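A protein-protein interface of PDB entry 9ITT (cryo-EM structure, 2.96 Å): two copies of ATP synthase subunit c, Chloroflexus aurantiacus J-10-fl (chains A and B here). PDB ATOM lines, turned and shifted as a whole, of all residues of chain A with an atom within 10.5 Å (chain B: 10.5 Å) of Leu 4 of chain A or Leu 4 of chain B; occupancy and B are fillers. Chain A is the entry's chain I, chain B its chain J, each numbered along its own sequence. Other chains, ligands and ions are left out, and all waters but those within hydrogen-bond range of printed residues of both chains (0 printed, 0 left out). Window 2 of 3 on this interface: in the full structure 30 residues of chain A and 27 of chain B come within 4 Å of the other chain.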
ATOM      1  N   GLY A   3      -6.135  20.799  37.083  1.00  0.00           N
ATOM      2  CA  GLY A   3      -4.917  21.479  36.701  1.00  0.00           C
ATOM      3  C   GLY A   3      -3.915  20.619  35.965  1.00  0.00           C
ATOM      4  O   GLY A   3      -2.760  21.029  35.813  1.00  0.00           O
ATOM      5  N   LEU A   4      -4.320  19.431  35.506  1.00  0.00           N
ATOM      6  CA  LEU A   4      -3.393  18.555  34.797  1.00  0.00           C
ATOM      7  C   LEU A   4      -2.890  19.208  33.517  1.00  0.00           C
ATOM      8  O   LEU A   4      -1.760  18.954  33.082  1.00  0.00           O
ATOM      9  CB  LEU A   4      -4.076  17.219  34.500  1.00  0.00           C
ATOM     10  CG  LEU A   4      -3.217  16.009  34.119  1.00  0.00           C
ATOM     11  CD1 LEU A   4      -2.121  15.735  35.136  1.00  0.00           C
ATOM     12  CD2 LEU A   4      -4.104  14.786  33.979  1.00  0.00           C
ATOM     13  N   ASN A   5      -3.711  20.055  32.895  1.00  0.00           N
ATOM     14  CA  ASN A   5      -3.227  20.834  31.760  1.00  0.00           C
ATOM     15  C   ASN A   5      -2.112  21.784  32.185  1.00  0.00           C
ATOM     16  O   ASN A   5      -1.112  21.941  31.472  1.00  0.00           O
ATOM     17  CB  ASN A   5      -4.377  21.612  31.117  1.00  0.00           C
ATOM     18  CG  ASN A   5      -5.154  22.445  32.119  1.00  0.00           C
ATOM     19  OD1 ASN A   5      -4.804  22.507  33.297  1.00  0.00           O
ATOM     20  ND2 ASN A   5      -6.216  23.093  31.654  1.00  0.00           N
ATOM     21  N   LEU A   6      -2.264  22.423  33.347  1.00  0.00           N
ATOM     22  CA  LEU A   6      -1.248  23.362  33.815  1.00  0.00           C
ATOM     23  C   LEU A   6       0.070  22.652  34.099  1.00  0.00           C
ATOM     24  O   LEU A   6       1.141  23.123  33.698  1.00  0.00           O
ATOM     25  CB  LEU A   6      -1.743  24.092  35.066  1.00  0.00           C
ATOM     26  CG  LEU A   6      -3.117  24.764  35.000  1.00  0.00           C
ATOM     27  CD1 LEU A   6      -3.376  25.558  36.273  1.00  0.00           C
ATOM     28  CD2 LEU A   6      -3.238  25.658  33.775  1.00  0.00           C
ATOM     29  N   VAL A   7       0.013  21.517  34.801  1.00  0.00           N
ATOM     30  CA  VAL A   7       1.243  20.799  35.114  1.00  0.00           C
ATOM     31  C   VAL A   7       1.849  20.213  33.847  1.00  0.00           C
ATOM     32  O   VAL A   7       3.072  20.125  33.720  1.00  0.00           O
ATOM     33  CB  VAL A   7       0.996  19.722  36.190  1.00  0.00           C
ATOM     34  CG1 VAL A   7       0.281  18.521  35.615  1.00  0.00           C
ATOM     35  CG2 VAL A   7       2.312  19.301  36.831  1.00  0.00           C
ATOM     36  N   ALA A   8       1.013  19.820  32.882  1.00  0.00           N
ATOM     37  CA  ALA A   8       1.541  19.358  31.602  1.00  0.00           C
ATOM     38  C   ALA A   8       2.305  20.472  30.892  1.00  0.00           C
ATOM     39  O   ALA A   8       3.425  20.265  30.411  1.00  0.00           O
ATOM     40  CB  ALA A   8       0.402  18.840  30.724  1.00  0.00           C
ATOM     41  N   THR A   9       1.714  21.667  30.825  1.00  0.00           N
ATOM     42  CA  THR A   9       2.386  22.794  30.183  1.00  0.00           C
ATOM     43  C   THR A   9       3.695  23.125  30.891  1.00  0.00           C
ATOM     44  O   THR A   9       4.735  23.335  30.245  1.00  0.00           O
ATOM     45  CB  THR A   9       1.459  24.012  30.181  1.00  0.00           C
ATOM     46  OG1 THR A   9       0.201  23.662  29.589  1.00  0.00           O
ATOM     47  CG2 THR A   9       2.073  25.169  29.407  1.00  0.00           C
ATOM     48  N   ALA A  10       3.658  23.171  32.223  1.00  0.00           N
ATOM     49  CA  ALA A  10       4.854  23.479  32.994  1.00  0.00           C
ATOM     50  C   ALA A  10       5.934  22.429  32.787  1.00  0.00           C
ATOM     51  O   ALA A  10       7.112  22.767  32.636  1.00  0.00           O
ATOM     52  CB  ALA A  10       4.500  23.588  34.473  1.00  0.00           C
ATOM     53  N   LEU A  11       5.555  21.150  32.791  1.00  0.00           N
ATOM     54  CA  LEU A  11       6.524  20.084  32.583  1.00  0.00           C
ATOM     55  C   LEU A  11       7.141  20.179  31.196  1.00  0.00           C
ATOM     56  O   LEU A  11       8.357  20.016  31.037  1.00  0.00           O
ATOM     57  CB  LEU A  11       5.845  18.729  32.786  1.00  0.00           C
ATOM     58  CG  LEU A  11       6.718  17.473  32.843  1.00  0.00           C
ATOM     59  CD1 LEU A  11       7.744  17.559  33.964  1.00  0.00           C
ATOM     60  CD2 LEU A  11       5.843  16.241  33.013  1.00  0.00           C
ATOM     61  N   ALA A  12       6.320  20.459  30.180  1.00  0.00           N
ATOM     62  CA  ALA A  12       6.840  20.620  28.827  1.00  0.00           C
ATOM     63  C   ALA A  12       7.886  21.724  28.775  1.00  0.00           C
ATOM     64  O   ALA A  12       9.010  21.509  28.304  1.00  0.00           O
ATOM     65  CB  ALA A  12       5.699  20.927  27.856  1.00  0.00           C
ATOM     66  N   ALA A  67       4.168  23.309  24.511  1.00  0.00           N
ATOM     67  CA  ALA A  67       3.615  23.774  25.778  1.00  0.00           C
ATOM     68  C   ALA A  67       2.509  24.798  25.556  1.00  0.00           C
ATOM     69  O   ALA A  67       1.476  24.764  26.234  1.00  0.00           O
ATOM     70  CB  ALA A  67       4.727  24.363  26.640  1.00  0.00           C
ATOM     71  N   ILE A  70      -0.626  23.007  24.409  1.00  0.00           N
ATOM     72  CA  ILE A  70      -1.284  22.329  25.525  1.00  0.00           C
ATOM     73  C   ILE A  70      -2.011  23.340  26.405  1.00  0.00           C
ATOM     74  O   ILE A  70      -3.182  23.156  26.759  1.00  0.00           O
ATOM     75  CB  ILE A  70      -0.260  21.511  26.337  1.00  0.00           C
ATOM     76  CG1 ILE A  70       0.281  20.326  25.520  1.00  0.00           C
ATOM     77  CG2 ILE A  70      -0.874  21.028  27.652  1.00  0.00           C
ATOM     78  CD1 ILE A  70      -0.739  19.239  25.179  1.00  0.00           C
ATOM     79  N   GLY A  71      -1.326  24.426  26.770  1.00  0.00           N
ATOM     80  CA  GLY A  71      -1.900  25.375  27.712  1.00  0.00           C
ATOM     81  C   GLY A  71      -3.100  26.121  27.162  1.00  0.00           C
ATOM     82  O   GLY A  71      -4.113  26.279  27.850  1.00  0.00           O
ATOM     83  N   GLY B   3      -6.883  14.642  31.176  1.00  0.00           N
ATOM     84  CA  GLY B   3      -5.723  15.356  30.673  1.00  0.00           C
ATOM     85  C   GLY B   3      -4.426  14.579  30.770  1.00  0.00           C
ATOM     86  O   GLY B   3      -3.344  15.163  30.653  1.00  0.00           O
ATOM     87  N   LEU B   4      -4.513  13.265  30.994  1.00  0.00           N
ATOM     88  CA  LEU B   4      -3.301  12.457  31.059  1.00  0.00           C
ATOM     89  C   LEU B   4      -2.562  12.459  29.727  1.00  0.00           C
ATOM     90  O   LEU B   4      -1.330  12.348  29.697  1.00  0.00           O
ATOM     91  CB  LEU B   4      -3.650  11.029  31.480  1.00  0.00           C
ATOM     92  CG  LEU B   4      -2.510  10.169  32.036  1.00  0.00           C
ATOM     93  CD1 LEU B   4      -1.936  10.752  33.321  1.00  0.00           C
ATOM     94  CD2 LEU B   4      -2.999   8.752  32.273  1.00  0.00           C
ATOM     95  N   ASN B   5      -3.294  12.590  28.619  1.00  0.00           N
ATOM     96  CA  ASN B   5      -2.645  12.730  27.320  1.00  0.00           C
ATOM     97  C   ASN B   5      -1.778  13.984  27.272  1.00  0.00           C
ATOM     98  O   ASN B   5      -0.703  13.981  26.664  1.00  0.00           O
ATOM     99  CB  ASN B   5      -3.693  12.764  26.205  1.00  0.00           C
ATOM    100  CG  ASN B   5      -4.784  13.787  26.457  1.00  0.00           C
ATOM    101  OD1 ASN B   5      -4.749  14.519  27.446  1.00  0.00           O
ATOM    102  ND2 ASN B   5      -5.762  13.841  25.562  1.00  0.00           N
ATOM    103  N   LEU B   6      -2.228  15.066  27.914  1.00  0.00           N
ATOM    104  CA  LEU B   6      -1.470  16.314  27.881  1.00  0.00           C
ATOM    105  C   LEU B   6      -0.130  16.163  28.591  1.00  0.00           C
ATOM    106  O   LEU B   6       0.919  16.538  28.051  1.00  0.00           O
ATOM    107  CB  LEU B   6      -2.286  17.446  28.514  1.00  0.00           C
ATOM    108  CG  LEU B   6      -3.770  17.559  28.153  1.00  0.00           C
ATOM    109  CD1 LEU B   6      -4.402  18.731  28.887  1.00  0.00           C
ATOM    110  CD2 LEU B   6      -3.958  17.697  26.650  1.00  0.00           C
ATOM    111  N   VAL B   7      -0.145  15.620  29.810  1.00  0.00           N
ATOM    112  CA  VAL B   7       1.108  15.435  30.536  1.00  0.00           C
ATOM    113  C   VAL B   7       1.972  14.391  29.843  1.00  0.00           C
ATOM    114  O   VAL B   7       3.204  14.483  29.874  1.00  0.00           O
ATOM    115  CB  VAL B   7       0.842  15.074  32.011  1.00  0.00           C
ATOM    116  CG1 VAL B   7       0.185  13.706  32.142  1.00  0.00           C
ATOM    117  CG2 VAL B   7       2.137  15.124  32.813  1.00  0.00           C
ATOM    118  N   ALA B   8       1.359  13.386  29.212  1.00  0.00           N
ATOM    119  CA  ALA B   8       2.134  12.423  28.436  1.00  0.00           C
ATOM    120  C   ALA B   8       2.882  13.116  27.303  1.00  0.00           C
ATOM    121  O   ALA B   8       4.082  12.891  27.104  1.00  0.00           O
ATOM    122  CB  ALA B   8       1.210  11.336  27.887  1.00  0.00           C
ATOM    123  N   THR B   9       2.185  13.976  26.556  1.00  0.00           N
ATOM    124  CA  THR B   9       2.824  14.721  25.476  1.00  0.00           C
ATOM    125  C   THR B   9       3.944  15.603  26.013  1.00  0.00           C
ATOM    126  O   THR B   9       5.036  15.665  25.431  1.00  0.00           O
ATOM    127  CB  THR B   9       1.777  15.571  24.750  1.00  0.00           C
ATOM    128  OG1 THR B   9       0.694  14.736  24.321  1.00  0.00           O
ATOM    129  CG2 THR B   9       2.374  16.268  23.536  1.00  0.00           C
ATOM    130  N   ALA B  10       3.685  16.295  27.123  1.00  0.00           N
ATOM    131  CA  ALA B  10       4.688  17.178  27.707  1.00  0.00           C
ATOM    132  C   ALA B  10       5.936  16.403  28.105  1.00  0.00           C
ATOM    133  O   ALA B  10       7.062  16.807  27.791  1.00  0.00           O
ATOM    134  CB  ALA B  10       4.097  17.892  28.919  1.00  0.00           C
ATOM    135  N   LEU B  11       5.748  15.281  28.802  1.00  0.00           N
ATOM    136  CA  LEU B  11       6.879  14.474  29.237  1.00  0.00           C
ATOM    137  C   LEU B  11       7.651  13.933  28.044  1.00  0.00           C
ATOM    138  O   LEU B  11       8.888  13.929  28.045  1.00  0.00           O
ATOM    139  CB  LEU B  11       6.381  13.334  30.127  1.00  0.00           C
ATOM    140  CG  LEU B  11       7.423  12.429  30.786  1.00  0.00           C
ATOM    141  CD1 LEU B  11       8.233  13.189  31.827  1.00  0.00           C
ATOM    142  CD2 LEU B  11       6.730  11.232  31.413  1.00  0.00           C
ATOM    143  N   ALA B  12       6.938  13.476  27.010  1.00  0.00           N
ATOM    144  CA  ALA B  12       7.608  12.950  25.827  1.00  0.00           C
ATOM    145  C   ALA B  12       8.472  14.018  25.168  1.00  0.00           C
ATOM    146  O   ALA B  12       9.645  13.775  24.860  1.00  0.00           O
ATOM    147  CB  ALA B  12       6.577  12.404  24.840  1.00  0.00           C
ATOM    148  N   ILE B  66       6.087  11.068  18.449  1.00  0.00           N
ATOM    149  CA  ILE B  66       5.199  10.383  19.387  1.00  0.00           C
ATOM    150  C   ILE B  66       4.382  11.399  20.176  1.00  0.00           C
ATOM    151  O   ILE B  66       3.200  11.180  20.471  1.00  0.00           O
ATOM    152  CB  ILE B  66       6.006   9.457  20.317  1.00  0.00           C
ATOM    153  CG1 ILE B  66       6.656   8.315  19.522  1.00  0.00           C
ATOM    154  CG2 ILE B  66       5.117   8.905  21.427  1.00  0.00           C
ATOM    155  CD1 ILE B  66       5.695   7.247  19.016  1.00  0.00           C
ATOM    156  N   ALA B  67       4.999  12.531  20.522  1.00  0.00           N
ATOM    157  CA  ALA B  67       4.287  13.578  21.245  1.00  0.00           C
ATOM    158  C   ALA B  67       3.131  14.133  20.425  1.00  0.00           C
ATOM    159  O   ALA B  67       2.034  14.338  20.951  1.00  0.00           O
ATOM    160  CB  ALA B  67       5.262  14.691  21.615  1.00  0.00           C
ATOM    161  N   ILE B  70       0.293  11.570  20.371  1.00  0.00           N
ATOM    162  CA  ILE B  70      -0.509  11.602  21.592  1.00  0.00           C
ATOM    163  C   ILE B  70      -1.373  12.859  21.632  1.00  0.00           C
ATOM    164  O   ILE B  70      -2.568  12.800  21.945  1.00  0.00           O
ATOM    165  CB  ILE B  70       0.396  11.507  22.837  1.00  0.00           C
ATOM    166  CG1 ILE B  70       1.173  10.181  22.871  1.00  0.00           C
ATOM    167  CG2 ILE B  70      -0.432  11.670  24.113  1.00  0.00           C
ATOM    168  CD1 ILE B  70       0.324   8.930  22.771  1.00  0.00           C
ATOM    169  N   GLY B  71      -0.784  14.014  21.315  1.00  0.00           N
ATOM    170  CA  GLY B  71      -1.489  15.272  21.496  1.00  0.00           C
ATOM    171  C   GLY B  71      -2.685  15.426  20.577  1.00  0.00           C
ATOM    172  O   GLY B  71      -3.742  15.903  20.999  1.00  0.00           O
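Leu 4 of chain A touches just these residues of chain B: Gly 3 (3.2 Å) and Leu 4 (3.4 Å).
Leu 4 of chain B touches just one residue of chain A: Leu 4.
Asn 5 of chain A touches just one residue of chain B: Leu 6.
No residue of chain B comes within 4 Å of Val 7 of chain A.
Leu 6 of chain B touches just these residues of chain A: Asn 5, Ala 8 and Ile 70.
Of chain A, only Ala 8 and Leu 11 come within 4 Å of Val 7 of chain B.
Of the printed residues of chain B, Leu 11 of chain A touches Val 7.
Printed residues of chain A within 4 Å of Ala 10 of chain B: Ala 8 (2.9 Å) and Ala 12 (3.6 Å).
Of the printed residues of chain B, Ala 12 of chain A touches Ala 10 (3.6 Å).
Gly 71 of chain A touches none of the printed residues of chain B.
Leu 6 of chain A touches none of the printed residues of chain B.
The nearest residue of chain B that does not touch Leu 4 of chain A is Val 7 of chain B (4.3 Å).
The nearest residue of chain A that does not touch Leu 4 of chain B is Ala 8 of chain A (6.8 Å).
The nearest printed residue of chain B that does not touch Ala 12 of chain A is Leu 11 of chain B (5.4 Å).
Among the printed residues, pairs that only touch across the chains: Leu 4 of chain A with Gly 3 of chain B (3.2 Å), Leu 4 of chain A with Leu 4 of chain B (3.4 Å), Asn 5 of chain A with Leu 6 of chain B (3.6 Å), Ala 8 of chain A with Leu 6 of chain B (3.5 Å), Ala 8 of chain A with Val 7 of chain B (3.4 Å), Ala 8 of chain A with Ala 10 of chain B (2.9 Å), Leu 11 of chain A with Val 7 of chain B (3.9 Å), Ala 12 of chain A with Ala 10 of chain B (3.6 Å) and Ile 70 of chain A with Leu 6 of chain B (3.9 Å).
Hydrophobic or aromatic side chains of chain A that line the printed part of chain B: Leu 4, Ala 8, Leu 11, Ala 12 and Ile 70.
Hydrophobic or aromatic side chains of chain B within 4 Å of the printed part of chain A: Leu 6, Val 7 and Ala 10.
Along chain B the printed residues that touch a printed residue of chain A span positions 3 to 10.
Among the printed residues, 9 pairs touch across the chains.
Leu 4 of chain A touches its own counterpart, Leu 4 of chain B.
Ala 8 of chain A touches Val 7 of chain B, but with the chains exchanged Val 7 of chain A does not touch Ala 8 of chain B (8.3 Å).
Ala 12 of chain A touches Ala 10 of chain B, but with the chains exchanged Ala 10 of chain A does not touch Ala 12 of chain B (10.7 Å).
Ile 70 of chain A touches Leu 6 of chain B, but with the chains exchanged Leu 6 of chain A does not touch Ile 70 of chain B (14.3 Å).
Positions printed for both chains: 3, 4, 5, 6, 7, 8, 9, 10, 11, 12, 67, 70 and 71.
Of the 9 pairs that touch across the chains among the printed residues, 1 has its exchanged pair printed and touching as well.
The backbone carbonyl oxygen (O) of Asn 5 of chain A lies within hydrogen-bond range of the side-chain hydroxyl (OG1) of Thr 9 of chain A (2.9 Å).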
